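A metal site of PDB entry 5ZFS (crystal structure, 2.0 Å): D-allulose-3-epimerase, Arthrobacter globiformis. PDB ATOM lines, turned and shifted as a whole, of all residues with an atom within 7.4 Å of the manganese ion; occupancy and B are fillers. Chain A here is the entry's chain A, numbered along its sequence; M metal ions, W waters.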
ATOM      1  N   HIS A   6      12.639 -22.123  26.818  1.00  0.00           N
ATOM      2  CA  HIS A   6      13.384 -20.909  27.103  1.00  0.00           C
ATOM      3  C   HIS A   6      12.443 -19.812  27.625  1.00  0.00           C
ATOM      4  O   HIS A   6      11.302 -19.705  27.175  1.00  0.00           O
ATOM      5  CB  HIS A   6      14.086 -20.450  25.828  1.00  0.00           C
ATOM      6  CG  HIS A   6      15.039 -19.317  26.013  1.00  0.00           C
ATOM      7  ND1 HIS A   6      14.658 -18.001  25.947  1.00  0.00           N
ATOM      8  CD2 HIS A   6      16.381 -19.304  26.235  1.00  0.00           C
ATOM      9  CE1 HIS A   6      15.705 -17.219  26.126  1.00  0.00           C
ATOM     10  NE2 HIS A   6      16.767 -17.984  26.305  1.00  0.00           N
ATOM     11  N   GLU A  35      14.597 -22.858  30.993  1.00  0.00           N
ATOM     12  CA  GLU A  35      15.916 -22.251  30.823  1.00  0.00           C
ATOM     13  C   GLU A  35      15.820 -20.744  31.086  1.00  0.00           C
ATOM     14  O   GLU A  35      15.163 -20.015  30.345  1.00  0.00           O
ATOM     15  CB  GLU A  35      16.447 -22.506  29.406  1.00  0.00           C
ATOM     16  CG  GLU A  35      17.788 -21.854  29.083  1.00  0.00           C
ATOM     17  CD  GLU A  35      18.239 -22.095  27.636  1.00  0.00           C
ATOM     18  OE1 GLU A  35      18.068 -23.232  27.139  1.00  0.00           O
ATOM     19  OE2 GLU A  35      18.771 -21.156  27.014  1.00  0.00           O
ATOM     20  N   SER A  63      21.083 -19.903  30.433  1.00  0.00           N
ATOM     21  CA  SER A  63      21.929 -19.526  29.319  1.00  0.00           C
ATOM     22  C   SER A  63      22.178 -18.026  29.390  1.00  0.00           C
ATOM     23  O   SER A  63      21.421 -17.284  30.021  1.00  0.00           O
ATOM     24  CB  SER A  63      21.268 -19.896  27.996  1.00  0.00           C
ATOM     25  OG  SER A  63      20.023 -19.226  27.823  1.00  0.00           O
ATOM     26  N   GLY A 104      25.540 -21.273  26.501  1.00  0.00           N
ATOM     27  CA  GLY A 104      25.279 -20.076  25.715  1.00  0.00           C
ATOM     28  C   GLY A 104      26.515 -19.567  25.000  1.00  0.00           C
ATOM     29  O   GLY A 104      27.479 -20.298  24.786  1.00  0.00           O
ATOM     30  N   VAL A 105      26.464 -18.295  24.636  1.00  0.00           N
ATOM     31  CA  VAL A 105      27.560 -17.654  23.935  1.00  0.00           C
ATOM     32  C   VAL A 105      28.458 -17.003  24.977  1.00  0.00           C
ATOM     33  O   VAL A 105      28.352 -15.809  25.260  1.00  0.00           O
ATOM     34  CB  VAL A 105      27.049 -16.618  22.927  1.00  0.00           C
ATOM     35  CG1 VAL A 105      28.217 -15.998  22.151  1.00  0.00           C
ATOM     36  CG2 VAL A 105      26.065 -17.278  21.964  1.00  0.00           C
ATOM     37  N   GLU A 146      27.524 -22.688  23.152  1.00  0.00           N
ATOM     38  CA  GLU A 146      26.535 -22.666  22.080  1.00  0.00           C
ATOM     39  C   GLU A 146      27.145 -22.186  20.770  1.00  0.00           C
ATOM     40  O   GLU A 146      27.612 -21.054  20.657  1.00  0.00           O
ATOM     41  CB  GLU A 146      25.341 -21.796  22.443  1.00  0.00           C
ATOM     42  CG  GLU A 146      24.252 -21.891  21.392  1.00  0.00           C
ATOM     43  CD  GLU A 146      23.041 -21.043  21.705  1.00  0.00           C
ATOM     44  OE1 GLU A 146      23.084 -20.222  22.647  1.00  0.00           O
ATOM     45  OE2 GLU A 146      22.035 -21.199  20.980  1.00  0.00           O
ATOM     46  N   VAL A 147      27.113 -23.072  19.780  1.00  0.00           N
ATOM     47  CA  VAL A 147      27.516 -22.726  18.420  1.00  0.00           C
ATOM     48  C   VAL A 147      26.422 -21.856  17.797  1.00  0.00           C
ATOM     49  O   VAL A 147      25.260 -22.264  17.713  1.00  0.00           O
ATOM     50  CB  VAL A 147      27.716 -24.008  17.583  1.00  0.00           C
ATOM     51  CG1 VAL A 147      28.068 -23.674  16.143  1.00  0.00           C
ATOM     52  CG2 VAL A 147      28.788 -24.878  18.227  1.00  0.00           C
ATOM     53  N   VAL A 148      26.791 -20.650  17.370  1.00  0.00           N
ATOM     54  CA  VAL A 148      25.823 -19.714  16.820  1.00  0.00           C
ATOM     55  C   VAL A 148      26.303 -19.168  15.477  1.00  0.00           C
ATOM     56  O   VAL A 148      27.467 -19.296  15.114  1.00  0.00           O
ATOM     57  CB  VAL A 148      25.548 -18.547  17.775  1.00  0.00           C
ATOM     58  CG1 VAL A 148      24.942 -19.059  19.080  1.00  0.00           C
ATOM     59  CG2 VAL A 148      26.808 -17.754  18.037  1.00  0.00           C
ATOM     60  N   GLU A 152      26.228 -13.614  15.100  1.00  0.00           N
ATOM     61  CA  GLU A 152      26.136 -13.598  16.553  1.00  0.00           C
ATOM     62  C   GLU A 152      27.466 -13.966  17.224  1.00  0.00           C
ATOM     63  O   GLU A 152      27.642 -13.729  18.412  1.00  0.00           O
ATOM     64  CB  GLU A 152      25.027 -14.550  17.039  1.00  0.00           C
ATOM     65  CG  GLU A 152      23.613 -14.068  16.704  1.00  0.00           C
ATOM     66  CD  GLU A 152      22.538 -14.845  17.426  1.00  0.00           C
ATOM     67  OE1 GLU A 152      22.818 -15.434  18.495  1.00  0.00           O
ATOM     68  OE2 GLU A 152      21.387 -14.879  16.913  1.00  0.00           O
ATOM     69  N   HIS A 177      26.787 -27.180  22.680  1.00  0.00           N
ATOM     70  CA  HIS A 177      25.371 -26.859  22.695  1.00  0.00           C
ATOM     71  C   HIS A 177      25.003 -26.489  21.249  1.00  0.00           C
ATOM     72  O   HIS A 177      25.517 -25.523  20.696  1.00  0.00           O
ATOM     73  CB  HIS A 177      25.157 -25.680  23.654  1.00  0.00           C
ATOM     74  CG  HIS A 177      23.810 -25.036  23.559  1.00  0.00           C
ATOM     75  ND1 HIS A 177      23.491 -23.906  24.277  1.00  0.00           N
ATOM     76  CD2 HIS A 177      22.718 -25.337  22.824  1.00  0.00           C
ATOM     77  CE1 HIS A 177      22.245 -23.546  24.005  1.00  0.00           C
ATOM     78  NE2 HIS A 177      21.761 -24.402  23.120  1.00  0.00           N
ATOM     79  N   LEU A 178      24.143 -27.286  20.632  1.00  0.00           N
ATOM     80  CA  LEU A 178      23.702 -27.052  19.269  1.00  0.00           C
ATOM     81  C   LEU A 178      22.275 -26.523  19.235  1.00  0.00           C
ATOM     82  O   LEU A 178      21.445 -26.882  20.079  1.00  0.00           O
ATOM     83  CB  LEU A 178      23.803 -28.336  18.437  1.00  0.00           C
ATOM     84  CG  LEU A 178      25.217 -28.790  18.099  1.00  0.00           C
ATOM     85  CD1 LEU A 178      25.178 -30.054  17.251  1.00  0.00           C
ATOM     86  CD2 LEU A 178      25.976 -27.679  17.396  1.00  0.00           C
ATOM     87  N   ASP A 179      22.012 -25.678  18.246  1.00  0.00           N
ATOM     88  CA  ASP A 179      20.724 -25.011  18.125  1.00  0.00           C
ATOM     89  C   ASP A 179      20.314 -25.115  16.648  1.00  0.00           C
ATOM     90  O   ASP A 179      21.060 -24.683  15.767  1.00  0.00           O
ATOM     91  CB  ASP A 179      20.857 -23.546  18.546  1.00  0.00           C
ATOM     92  CG  ASP A 179      19.573 -22.737  18.361  1.00  0.00           C
ATOM     93  OD1 ASP A 179      18.670 -23.179  17.623  1.00  0.00           O
ATOM     94  OD2 ASP A 179      19.475 -21.649  18.946  1.00  0.00           O
ATOM     95  N   THR A 180      19.153 -25.701  16.397  1.00  0.00           N
ATOM     96  CA  THR A 180      18.760 -26.000  15.020  1.00  0.00           C
ATOM     97  C   THR A 180      18.659 -24.731  14.190  1.00  0.00           C
ATOM     98  O   THR A 180      18.929 -24.734  12.978  1.00  0.00           O
ATOM     99  CB  THR A 180      17.417 -26.755  14.964  1.00  0.00           C
ATOM    100  OG1 THR A 180      16.395 -25.957  15.565  1.00  0.00           O
ATOM    101  CG2 THR A 180      17.519 -28.071  15.700  1.00  0.00           C
ATOM    102  N   TYR A 181      18.276 -23.633  14.837  1.00  0.00           N
ATOM    103  CA  TYR A 181      18.158 -22.352  14.150  1.00  0.00           C
ATOM    104  C   TYR A 181      19.504 -21.914  13.569  1.00  0.00           C
ATOM    105  O   TYR A 181      19.573 -21.393  12.454  1.00  0.00           O
ATOM    106  CB  TYR A 181      17.643 -21.295  15.116  1.00  0.00           C
ATOM    107  CG  TYR A 181      17.867 -19.862  14.656  1.00  0.00           C
ATOM    108  CD1 TYR A 181      17.029 -19.283  13.718  1.00  0.00           C
ATOM    109  CD2 TYR A 181      18.901 -19.106  15.184  1.00  0.00           C
ATOM    110  CE1 TYR A 181      17.231 -17.970  13.304  1.00  0.00           C
ATOM    111  CE2 TYR A 181      19.107 -17.797  14.778  1.00  0.00           C
ATOM    112  CZ  TYR A 181      18.267 -17.239  13.842  1.00  0.00           C
ATOM    113  OH  TYR A 181      18.473 -15.930  13.437  1.00  0.00           O
ATOM    114  N   HIS A 182      20.567 -22.123  14.333  1.00  0.00           N
ATOM    115  CA  HIS A 182      21.922 -21.751  13.906  1.00  0.00           C
ATOM    116  C   HIS A 182      22.527 -22.789  12.959  1.00  0.00           C
ATOM    117  O   HIS A 182      23.263 -22.428  12.037  1.00  0.00           O
ATOM    118  CB  HIS A 182      22.833 -21.572  15.117  1.00  0.00           C
ATOM    119  CG  HIS A 182      22.454 -20.402  15.974  1.00  0.00           C
ATOM    120  ND1 HIS A 182      22.510 -19.103  15.520  1.00  0.00           N
ATOM    121  CD2 HIS A 182      21.987 -20.342  17.248  1.00  0.00           C
ATOM    122  CE1 HIS A 182      22.098 -18.290  16.480  1.00  0.00           C
ATOM    123  NE2 HIS A 182      21.784 -19.018  17.539  1.00  0.00           N
ATOM    124  N   VAL A 204      20.790 -28.973  23.641  1.00  0.00           N
ATOM    125  CA  VAL A 204      20.165 -28.742  22.341  1.00  0.00           C
ATOM    126  C   VAL A 204      19.045 -27.713  22.455  1.00  0.00           C
ATOM    127  O   VAL A 204      18.202 -27.803  23.338  1.00  0.00           O
ATOM    128  CB  VAL A 204      19.583 -30.051  21.778  1.00  0.00           C
ATOM    129  CG1 VAL A 204      18.549 -29.770  20.707  1.00  0.00           C
ATOM    130  CG2 VAL A 204      20.699 -30.935  21.239  1.00  0.00           C
ATOM    131  N   HIS A 205      19.052 -26.739  21.535  1.00  0.00           N
ATOM    132  CA  HIS A 205      17.912 -25.853  21.339  1.00  0.00           C
ATOM    133  C   HIS A 205      17.159 -26.230  20.062  1.00  0.00           C
ATOM    134  O   HIS A 205      17.763 -26.482  19.019  1.00  0.00           O
ATOM    135  CB  HIS A 205      18.371 -24.391  21.211  1.00  0.00           C
ATOM    136  CG  HIS A 205      18.508 -23.683  22.521  1.00  0.00           C
ATOM    137  ND1 HIS A 205      19.048 -22.414  22.622  1.00  0.00           N
ATOM    138  CD2 HIS A 205      18.188 -24.058  23.786  1.00  0.00           C
ATOM    139  CE1 HIS A 205      19.051 -22.035  23.890  1.00  0.00           C
ATOM    140  NE2 HIS A 205      18.540 -23.015  24.613  1.00  0.00           N
ATOM    141  N   ILE A 206      15.840 -26.258  20.189  1.00  0.00           N
ATOM    142  CA  ILE A 206      14.943 -26.483  19.068  1.00  0.00           C
ATOM    143  C   ILE A 206      14.337 -25.148  18.679  1.00  0.00           C
ATOM    144  O   ILE A 206      13.472 -24.619  19.394  1.00  0.00           O
ATOM    145  CB  ILE A 206      13.829 -27.458  19.462  1.00  0.00           C
ATOM    146  CG1 ILE A 206      14.436 -28.779  19.941  1.00  0.00           C
ATOM    147  CG2 ILE A 206      12.857 -27.678  18.303  1.00  0.00           C
ATOM    148  CD1 ILE A 206      15.379 -29.416  18.941  1.00  0.00           C
ATOM    149  N   GLY A 207      14.795 -24.593  17.561  1.00  0.00           N
ATOM    150  CA  GLY A 207      14.244 -23.357  17.019  1.00  0.00           C
ATOM    151  C   GLY A 207      13.996 -23.442  15.520  1.00  0.00           C
ATOM    152  O   GLY A 207      14.803 -23.976  14.779  1.00  0.00           O
ATOM    153  N   ARG A 211      12.650 -18.570  14.040  1.00  0.00           N
ATOM    154  CA  ARG A 211      12.476 -18.558  15.489  1.00  0.00           C
ATOM    155  C   ARG A 211      11.034 -18.332  15.942  1.00  0.00           C
ATOM    156  O   ARG A 211      10.795 -17.911  17.069  1.00  0.00           O
ATOM    157  CB  ARG A 211      13.408 -17.534  16.150  1.00  0.00           C
ATOM    158  CG  ARG A 211      14.833 -17.595  15.653  1.00  0.00           C
ATOM    159  CD  ARG A 211      15.782 -16.844  16.579  1.00  0.00           C
ATOM    160  NE  ARG A 211      16.532 -17.753  17.432  1.00  0.00           N
ATOM    161  CZ  ARG A 211      17.696 -17.439  17.989  1.00  0.00           C
ATOM    162  NH1 ARG A 211      18.218 -16.237  17.781  1.00  0.00           N
ATOM    163  NH2 ARG A 211      18.330 -18.312  18.754  1.00  0.00           N
ATOM    164  N   VAL A 238      15.419 -28.208  24.313  1.00  0.00           N
ATOM    165  CA  VAL A 238      14.791 -27.008  24.838  1.00  0.00           C
ATOM    166  C   VAL A 238      14.275 -26.135  23.694  1.00  0.00           C
ATOM    167  O   VAL A 238      15.036 -25.769  22.799  1.00  0.00           O
ATOM    168  CB  VAL A 238      15.774 -26.191  25.699  1.00  0.00           C
ATOM    169  CG1 VAL A 238      15.126 -24.880  26.144  1.00  0.00           C
ATOM    170  CG2 VAL A 238      16.247 -26.999  26.892  1.00  0.00           C
ATOM    171  N   GLU A 240      13.156 -22.822  21.873  1.00  0.00           N
ATOM    172  CA  GLU A 240      13.469 -21.398  21.940  1.00  0.00           C
ATOM    173  C   GLU A 240      12.744 -20.671  20.812  1.00  0.00           C
ATOM    174  O   GLU A 240      12.765 -21.109  19.660  1.00  0.00           O
ATOM    175  CB  GLU A 240      14.985 -21.175  21.824  1.00  0.00           C
ATOM    176  CG  GLU A 240      15.408 -19.736  21.995  1.00  0.00           C
ATOM    177  CD  GLU A 240      16.915 -19.563  22.037  1.00  0.00           C
ATOM    178  OE1 GLU A 240      17.591 -20.127  21.158  1.00  0.00           O
ATOM    179  OE2 GLU A 240      17.419 -18.868  22.953  1.00  0.00           O
ATOM    180  N   PHE A 242      11.213 -16.406  19.674  1.00  0.00           N
ATOM    181  CA  PHE A 242      11.228 -14.964  19.955  1.00  0.00           C
ATOM    182  C   PHE A 242      10.236 -14.254  19.047  1.00  0.00           C
ATOM    183  O   PHE A 242      10.194 -14.496  17.837  1.00  0.00           O
ATOM    184  CB  PHE A 242      12.638 -14.392  19.731  1.00  0.00           C
ATOM    185  CG  PHE A 242      13.693 -15.010  20.597  1.00  0.00           C
ATOM    186  CD1 PHE A 242      13.841 -14.610  21.922  1.00  0.00           C
ATOM    187  CD2 PHE A 242      14.519 -15.986  20.098  1.00  0.00           C
ATOM    188  CE1 PHE A 242      14.808 -15.178  22.730  1.00  0.00           C
ATOM    189  CE2 PHE A 242      15.492 -16.565  20.898  1.00  0.00           C
ATOM    190  CZ  PHE A 242      15.636 -16.161  22.215  1.00  0.00           C
ATOM    191  N   LEU A 255      19.280 -10.014  19.266  1.00  0.00           N
ATOM    192  CA  LEU A 255      18.963 -11.123  18.371  1.00  0.00           C
ATOM    193  C   LEU A 255      18.164 -10.653  17.162  1.00  0.00           C
ATOM    194  O   LEU A 255      17.794 -11.457  16.304  1.00  0.00           O
ATOM    195  CB  LEU A 255      18.185 -12.209  19.118  1.00  0.00           C
ATOM    196  CG  LEU A 255      18.950 -12.889  20.263  1.00  0.00           C
ATOM    197  CD1 LEU A 255      18.114 -14.001  20.879  1.00  0.00           C
ATOM    198  CD2 LEU A 255      20.275 -13.446  19.759  1.00  0.00           C
HETATM  199 MN    MN M   1      19.952 -20.737  21.148  1.00  0.00          MN
HETATM  200  O   HOH W   1      20.331 -18.720  22.902  1.00  0.00           O
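N of Glu 146 sits at hydrogen-bond distance from O of Gly 104 (2.9 Å). NE2 of His 177 lies close to ND1 of His 205, at 3.4 Å. N of His 205 sits at hydrogen-bond distance from O of Leu 178 (2.8 Å). O of His 205 is in hydrogen-bond range of N of Thr 180 (3.1 Å). The side-chain carboxylate (OD1) of Asp 179 sits at hydrogen-bond distance from the backbone NH (N) of Tyr 181, 2.9 Å away. OE1 of Glu 240 lies close to NH2 of Arg 211 (3.1 Å). O of Arg 211 is in hydrogen-bond range of N of Phe 242. The guanidinium group (NH1) of Arg 211 is in salt-bridge range of the side-chain carboxylate (OE2) of Glu 152 (3.6 Å).
Arg 211 touches the manganese ion. Of the 24 residues printed, 5 come within 4 Å of the manganese ion.
The manganese ion is bound by the side-chain carboxylate (OE2) of Glu 146, a ring nitrogen (ND1) of His 205, the side-chain carboxylate (OD2) of Asp 179, the side-chain carboxylate (OE1) of Glu 240 and water W1. The manganese ion has five donor atoms within binding distance.
Water W1 lies within hydrogen-bond range of OE2 of Glu 240 (2.9 Å) and OE1 of Glu 146 (3.1 Å).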
